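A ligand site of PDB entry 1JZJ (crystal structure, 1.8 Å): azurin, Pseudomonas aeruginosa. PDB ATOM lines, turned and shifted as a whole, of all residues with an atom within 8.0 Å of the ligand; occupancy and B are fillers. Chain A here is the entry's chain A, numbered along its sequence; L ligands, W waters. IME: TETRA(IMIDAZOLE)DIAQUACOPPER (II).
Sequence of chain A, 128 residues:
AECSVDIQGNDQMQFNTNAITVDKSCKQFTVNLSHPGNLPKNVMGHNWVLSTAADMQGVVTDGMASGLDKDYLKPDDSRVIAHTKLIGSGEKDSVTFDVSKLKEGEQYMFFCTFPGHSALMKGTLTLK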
ATOM      1  N   VAL A  22      21.712 -18.751  16.565  1.00  0.00           N
ATOM      2  CA  VAL A  22      21.715 -17.305  16.352  1.00  0.00           C
ATOM      3  C   VAL A  22      21.016 -16.658  17.532  1.00  0.00           C
ATOM      4  O   VAL A  22      19.876 -16.994  17.853  1.00  0.00           O
ATOM      5  CB  VAL A  22      20.981 -16.920  15.051  1.00  0.00           C
ATOM      6  CG1 VAL A  22      20.905 -15.404  14.915  1.00  0.00           C
ATOM      7  CG2 VAL A  22      21.691 -17.519  13.852  1.00  0.00           C
ATOM      8  N   ASP A  23      21.708 -15.730  18.184  1.00  0.00           N
ATOM      9  CA  ASP A  23      21.138 -15.039  19.344  1.00  0.00           C
ATOM     10  C   ASP A  23      20.105 -14.003  18.915  1.00  0.00           C
ATOM     11  O   ASP A  23      20.309 -13.276  17.944  1.00  0.00           O
ATOM     12  CB  ASP A  23      22.244 -14.364  20.156  1.00  0.00           C
ATOM     13  CG  ASP A  23      21.774 -13.926  21.518  1.00  0.00           C
ATOM     14  OD1 ASP A  23      21.323 -12.770  21.651  1.00  0.00           O
ATOM     15  OD2 ASP A  23      21.832 -14.739  22.458  1.00  0.00           O
ATOM     16  N   LYS A  24      19.012 -13.928  19.667  1.00  0.00           N
ATOM     17  CA  LYS A  24      17.932 -12.989  19.374  1.00  0.00           C
ATOM     18  C   LYS A  24      18.314 -11.521  19.455  1.00  0.00           C
ATOM     19  O   LYS A  24      17.640 -10.679  18.862  1.00  0.00           O
ATOM     20  CB  LYS A  24      16.737 -13.222  20.298  1.00  0.00           C
ATOM     21  CG  LYS A  24      16.256 -14.646  20.382  1.00  0.00           C
ATOM     22  CD  LYS A  24      14.820 -14.707  20.875  1.00  0.00           C
ATOM     23  CE  LYS A  24      14.570 -13.858  22.107  1.00  0.00           C
ATOM     24  NZ  LYS A  24      15.228 -14.395  23.324  1.00  0.00           N
ATOM     25  N   SER A  25      19.368 -11.183  20.202  1.00  0.00           N
ATOM     26  CA  SER A  25      19.783  -9.791  20.311  1.00  0.00           C
ATOM     27  C   SER A  25      20.346  -9.277  18.983  1.00  0.00           C
ATOM     28  O   SER A  25      20.381  -8.081  18.743  1.00  0.00           O
ATOM     29  CB  SER A  25      20.818  -9.598  21.430  1.00  0.00           C
ATOM     30  OG  SER A  25      22.077 -10.136  21.071  1.00  0.00           O
ATOM     31  N   CYS A  26      20.739 -10.210  18.123  1.00  0.00           N
ATOM     32  CA  CYS A  26      21.307  -9.867  16.812  1.00  0.00           C
ATOM     33  C   CYS A  26      20.252  -9.417  15.814  1.00  0.00           C
ATOM     34  O   CYS A  26      19.218 -10.072  15.660  1.00  0.00           O
ATOM     35  CB  CYS A  26      22.053 -11.059  16.221  1.00  0.00           C
ATOM     36  SG  CYS A  26      23.432 -11.699  17.230  1.00  0.00           S
ATOM     37  N   LYS A  27      20.510  -8.297  15.153  1.00  0.00           N
ATOM     38  CA  LYS A  27      19.610  -7.786  14.126  1.00  0.00           C
ATOM     39  C   LYS A  27      20.108  -8.334  12.794  1.00  0.00           C
ATOM     40  O   LYS A  27      19.335  -8.535  11.866  1.00  0.00           O
ATOM     41  CB  LYS A  27      19.616  -6.259  14.112  1.00  0.00           C
ATOM     42  CG  LYS A  27      18.963  -5.668  15.337  1.00  0.00           C
ATOM     43  CD  LYS A  27      18.663  -4.198  15.148  1.00  0.00           C
ATOM     44  CE  LYS A  27      17.395  -3.834  15.899  1.00  0.00           C
ATOM     45  NZ  LYS A  27      17.133  -2.373  15.883  1.00  0.00           N
ATOM     46  N   GLN A  28      21.416  -8.551  12.734  1.00  0.00           N
ATOM     47  CA  GLN A  28      22.080  -9.100  11.563  1.00  0.00           C
ATOM     48  C   GLN A  28      22.982 -10.233  12.036  1.00  0.00           C
ATOM     49  O   GLN A  28      23.438 -10.233  13.189  1.00  0.00           O
ATOM     50  CB  GLN A  28      22.943  -8.048  10.880  1.00  0.00           C
ATOM     51  CG  GLN A  28      22.190  -6.931  10.189  1.00  0.00           C
ATOM     52  CD  GLN A  28      23.126  -5.935   9.528  1.00  0.00           C
ATOM     53  OE1 GLN A  28      24.039  -5.415  10.175  1.00  0.00           O
ATOM     54  NE2 GLN A  28      22.908  -5.684   8.249  1.00  0.00           N
ATOM     55  N   PHE A  29      23.230 -11.195  11.156  1.00  0.00           N
ATOM     56  CA  PHE A  29      24.094 -12.314  11.477  1.00  0.00           C
ATOM     57  C   PHE A  29      25.050 -12.507  10.303  1.00  0.00           C
ATOM     58  O   PHE A  29      24.647 -12.360   9.145  1.00  0.00           O
ATOM     59  CB  PHE A  29      23.277 -13.586  11.718  1.00  0.00           C
ATOM     60  CG  PHE A  29      24.068 -14.717  12.301  1.00  0.00           C
ATOM     61  CD1 PHE A  29      24.457 -14.689  13.639  1.00  0.00           C
ATOM     62  CD2 PHE A  29      24.429 -15.803  11.528  1.00  0.00           C
ATOM     63  CE1 PHE A  29      25.199 -15.735  14.184  1.00  0.00           C
ATOM     64  CE2 PHE A  29      25.162 -16.858  12.061  1.00  0.00           C
ATOM     65  CZ  PHE A  29      25.556 -16.822  13.397  1.00  0.00           C
ATOM     66  N   PHE A  97      23.050 -11.356   6.967  1.00  0.00           N
ATOM     67  CA  PHE A  97      21.619 -11.335   6.722  1.00  0.00           C
ATOM     68  C   PHE A  97      20.798 -10.828   7.898  1.00  0.00           C
ATOM     69  O   PHE A  97      21.267 -10.803   9.032  1.00  0.00           O
ATOM     70  CB  PHE A  97      21.114 -12.720   6.277  1.00  0.00           C
ATOM     71  CG  PHE A  97      21.187 -13.772   7.343  1.00  0.00           C
ATOM     72  CD1 PHE A  97      22.306 -14.596   7.450  1.00  0.00           C
ATOM     73  CD2 PHE A  97      20.130 -13.972   8.222  1.00  0.00           C
ATOM     74  CE1 PHE A  97      22.365 -15.600   8.415  1.00  0.00           C
ATOM     75  CE2 PHE A  97      20.176 -14.981   9.183  1.00  0.00           C
ATOM     76  CZ  PHE A  97      21.295 -15.797   9.276  1.00  0.00           C
ATOM     77  N   ASP A  98      19.566 -10.428   7.590  1.00  0.00           N
ATOM     78  CA  ASP A  98      18.615  -9.916   8.571  1.00  0.00           C
ATOM     79  C   ASP A  98      18.028 -11.063   9.375  1.00  0.00           C
ATOM     80  O   ASP A  98      17.355 -11.932   8.819  1.00  0.00           O
ATOM     81  CB  ASP A  98      17.505  -9.172   7.830  1.00  0.00           C
ATOM     82  CG  ASP A  98      16.606  -8.375   8.760  1.00  0.00           C
ATOM     83  OD1 ASP A  98      16.657  -8.574   9.995  1.00  0.00           O
ATOM     84  OD2 ASP A  98      15.848  -7.520   8.245  1.00  0.00           O
ATOM     85  N   VAL A  99      18.220 -11.020  10.686  1.00  0.00           N
ATOM     86  CA  VAL A  99      17.706 -12.060  11.584  1.00  0.00           C
ATOM     87  C   VAL A  99      16.184 -12.083  11.681  1.00  0.00           C
ATOM     88  O   VAL A  99      15.605 -13.082  12.093  1.00  0.00           O
ATOM     89  CB  VAL A  99      18.330 -11.940  12.993  1.00  0.00           C
ATOM     90  CG1 VAL A  99      17.878 -13.099  13.880  1.00  0.00           C
ATOM     91  CG2 VAL A  99      19.844 -11.938  12.892  1.00  0.00           C
ATOM     92  N   SER A 100      15.543 -10.985  11.281  1.00  0.00           N
ATOM     93  CA  SER A 100      14.084 -10.902  11.326  1.00  0.00           C
ATOM     94  C   SER A 100      13.429 -11.852  10.320  1.00  0.00           C
ATOM     95  O   SER A 100      12.206 -11.987  10.271  1.00  0.00           O
ATOM     96  CB  SER A 100      13.600  -9.466  11.092  1.00  0.00           C
ATOM     97  OG  SER A 100      13.979  -8.989   9.817  1.00  0.00           O
ATOM     98  N   LYS A 101      14.263 -12.505   9.506  1.00  0.00           N
ATOM     99  CA  LYS A 101      13.776 -13.474   8.529  1.00  0.00           C
ATOM    100  C   LYS A 101      13.677 -14.838   9.231  1.00  0.00           C
ATOM    101  O   LYS A 101      13.268 -15.834   8.630  1.00  0.00           O
ATOM    102  CB  LYS A 101      14.740 -13.565   7.343  1.00  0.00           C
ATOM    103  CG  LYS A 101      14.718 -12.339   6.437  1.00  0.00           C
ATOM    104  CD  LYS A 101      15.831 -12.394   5.410  1.00  0.00           C
ATOM    105  CE  LYS A 101      15.830 -11.168   4.512  1.00  0.00           C
ATOM    106  NZ  LYS A 101      14.695 -11.184   3.548  1.00  0.00           N
ATOM    107  N   LEU A 102      14.055 -14.844  10.499  1.00  0.00           N
ATOM    108  CA  LEU A 102      14.017 -16.052  11.313  1.00  0.00           C
ATOM    109  C   LEU A 102      13.066 -15.851  12.485  1.00  0.00           C
ATOM    110  O   LEU A 102      12.803 -14.730  12.899  1.00  0.00           O
ATOM    111  CB  LEU A 102      15.413 -16.357  11.864  1.00  0.00           C
ATOM    112  CG  LEU A 102      16.618 -16.333  10.918  1.00  0.00           C
ATOM    113  CD1 LEU A 102      17.880 -16.692  11.692  1.00  0.00           C
ATOM    114  CD2 LEU A 102      16.418 -17.304   9.759  1.00  0.00           C
ATOM    115  N   LYS A 103      12.552 -16.966  13.005  1.00  0.00           N
ATOM    116  CA  LYS A 103      11.655 -16.941  14.156  1.00  0.00           C
ATOM    117  C   LYS A 103      11.942 -18.180  14.984  1.00  0.00           C
ATOM    118  O   LYS A 103      12.566 -19.125  14.518  1.00  0.00           O
ATOM    119  CB  LYS A 103      10.179 -16.973  13.718  1.00  0.00           C
ATOM    120  CG  LYS A 103       9.703 -18.330  13.212  1.00  0.00           C
ATOM    121  CD  LYS A 103       8.215 -18.348  12.904  1.00  0.00           C
ATOM    122  CE  LYS A 103       7.759 -19.736  12.481  1.00  0.00           C
ATOM    123  NZ  LYS A 103       6.316 -19.775  12.107  1.00  0.00           N
ATOM    124  N   GLU A 104      11.519 -18.151  16.249  1.00  0.00           N
ATOM    125  CA  GLU A 104      11.702 -19.300  17.110  1.00  0.00           C
ATOM    126  C   GLU A 104      10.598 -20.289  16.740  1.00  0.00           C
ATOM    127  O   GLU A 104       9.549 -19.888  16.231  1.00  0.00           O
ATOM    128  CB  GLU A 104      11.533 -18.904  18.576  1.00  0.00           C
ATOM    129  CG  GLU A 104      12.518 -17.868  19.065  1.00  0.00           C
ATOM    130  CD  GLU A 104      12.603 -17.838  20.590  1.00  0.00           C
ATOM    131  OE1 GLU A 104      12.517 -16.726  21.163  1.00  0.00           O
ATOM    132  OE2 GLU A 104      12.754 -18.913  21.200  1.00  0.00           O
ATOM    133  N   TYR A 108      15.612 -24.401  10.629  1.00  0.00           N
ATOM    134  CA  TYR A 108      16.300 -23.912   9.447  1.00  0.00           C
ATOM    135  C   TYR A 108      17.475 -24.844   9.204  1.00  0.00           C
ATOM    136  O   TYR A 108      17.978 -25.468  10.131  1.00  0.00           O
ATOM    137  CB  TYR A 108      16.811 -22.474   9.666  1.00  0.00           C
ATOM    138  CG  TYR A 108      15.714 -21.504   9.980  1.00  0.00           C
ATOM    139  CD1 TYR A 108      14.858 -21.029   8.976  1.00  0.00           C
ATOM    140  CD2 TYR A 108      15.476 -21.087  11.290  1.00  0.00           C
ATOM    141  CE1 TYR A 108      13.799 -20.174   9.280  1.00  0.00           C
ATOM    142  CE2 TYR A 108      14.425 -20.235  11.598  1.00  0.00           C
ATOM    143  CZ  TYR A 108      13.586 -19.785  10.590  1.00  0.00           C
ATOM    144  OH  TYR A 108      12.525 -18.966  10.887  1.00  0.00           O
ATOM    145  N   LEU A 127      17.205 -19.875  15.971  1.00  0.00           N
ATOM    146  CA  LEU A 127      17.179 -18.558  16.595  1.00  0.00           C
ATOM    147  C   LEU A 127      16.835 -18.792  18.070  1.00  0.00           C
ATOM    148  O   LEU A 127      15.783 -19.365  18.367  1.00  0.00           O
ATOM    149  CB  LEU A 127      16.105 -17.682  15.945  1.00  0.00           C
ATOM    150  CG  LEU A 127      15.847 -16.317  16.583  1.00  0.00           C
ATOM    151  CD1 LEU A 127      17.069 -15.430  16.434  1.00  0.00           C
ATOM    152  CD2 LEU A 127      14.648 -15.665  15.925  1.00  0.00           C
ATOM    153  N   LYS A 128      17.705 -18.353  18.978  1.00  0.00           N
ATOM    154  CA  LYS A 128      17.450 -18.546  20.409  1.00  0.00           C
ATOM    155  C   LYS A 128      17.865 -17.406  21.332  1.00  0.00           C
ATOM    156  O   LYS A 128      17.191 -17.228  22.363  1.00  0.00           O
ATOM    157  CB  LYS A 128      18.073 -19.859  20.885  1.00  0.00           C
ATOM    158  CG  LYS A 128      17.316 -21.086  20.393  1.00  0.00           C
ATOM    159  CD  LYS A 128      18.196 -22.307  20.272  1.00  0.00           C
ATOM    160  CE  LYS A 128      18.466 -22.945  21.623  1.00  0.00           C
ATOM    161  NZ  LYS A 128      19.299 -24.170  21.451  1.00  0.00           N
ATOM    162  OXT LYS A 128      18.853 -16.694  21.023  1.00  0.00           O
HETATM  163 CU   IME L   1      14.562  -8.970  16.599  1.00  0.00          CU
HETATM  164  O1  IME L   1      12.306  -7.902  16.630  1.00  0.00           O
HETATM  165  O2  IME L   1      16.582 -10.432  16.516  1.00  0.00           O
HETATM  166  CG1 IME L   1      11.968 -11.654  14.518  1.00  0.00           C
HETATM  167  CDC IME L   1      12.292 -10.409  14.948  1.00  0.00           C
HETATM  168  NDB IME L   1      13.127 -12.366  14.751  1.00  0.00           N
HETATM  169  CEB IME L   1      14.113 -11.676  15.283  1.00  0.00           C
HETATM  170  NEC IME L   1      13.592 -10.463  15.407  1.00  0.00           N
HETATM  171  CG2 IME L   1      13.985 -10.340  20.412  1.00  0.00           C
HETATM  172  CDM IME L   1      14.687  -9.854  19.368  1.00  0.00           C
HETATM  173  NDL IME L   1      12.704 -10.320  19.918  1.00  0.00           N
HETATM  174  CEL IME L   1      12.737  -9.859  18.681  1.00  0.00           C
HETATM  175  NEM IME L   1      13.948  -9.544  18.256  1.00  0.00           N
HETATM  176  CG3 IME L   1      17.109  -6.362  18.533  1.00  0.00           C
HETATM  177  CDW IME L   1      16.855  -7.573  17.982  1.00  0.00           C
HETATM  178  NDV IME L   1      15.997  -5.554  18.483  1.00  0.00           N
HETATM  179  CEV IME L   1      15.079  -6.301  17.900  1.00  0.00           C
HETATM  180  NEW IME L   1      15.537  -7.506  17.581  1.00  0.00           N
HETATM  181  CG4 IME L   1      15.748  -6.892  13.051  1.00  0.00           C
HETATM  182  CD6 IME L   1      15.108  -6.894  14.246  1.00  0.00           C
HETATM  183  ND5 IME L   1      16.326  -8.130  12.880  1.00  0.00           N
HETATM  184  CE5 IME L   1      16.045  -8.873  13.935  1.00  0.00           C
HETATM  185  NE6 IME L   1      15.320  -8.142  14.765  1.00  0.00           N
HETATM  186  O   HOH W   1      16.262  -4.182  12.421  1.00  0.00           O
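The side-chain amino group of Lys 24 is in salt-bridge range of the chain-end carboxylate of Lys 128 (3.6 Å).
The side-chain carboxylate (OD1) of Asp 98 is in hydrogen-bond range of the side-chain hydroxyl (OG) of Ser 100 (2.7 Å).
The backbone NH of Val 99 is in hydrogen-bond range of the backbone carbonyl oxygen of Lys 27, 3.0 Å away.
The side-chain hydroxyl (OG) of Ser 25 is in hydrogen-bond range of the side-chain carboxylate (OD1) of Asp 23.
The backbone carbonyl oxygen (O) of Lys 24 sits close to an oxygen (O2) of the ligand (2.6 Å).
ND5 of the ligand sits at hydrogen-bond distance from N of Ser 100, 3.4 Å away.
O of Cys 26 sits close to O2 of the ligand (2.8 Å).
O of Lys 27 sits close to ND5 of the ligand (3.2 Å).
The side-chain carboxylate (OD1) of Asp 98 lies close to a nitrogen (ND5) of the ligand (2.9 Å).
A nitrogen (NDB) of the ligand lies close to the backbone carbonyl oxygen (O) of Leu 102, at 3.0 Å.
O of Ser 25 touches CDW of the ligand (3.6 Å).
Val 99 touches the ligand (O to NDB, 3.7 Å).
CD2 of Leu 127 touches NDB of the ligand, at 3.8 Å.
Hydrophobic or aromatic side chains that line the ligand: Val 99 and Leu 127.
Nine residues have an atom within 4 Å of the ligand: Lys 24, Ser 25, Cys 26, Lys 27, Asp 98, Val 99, Ser 100, Leu 102 and Leu 127.
The nearest printed residue that does not touch the ligand is Lys 103 (4.8 Å).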
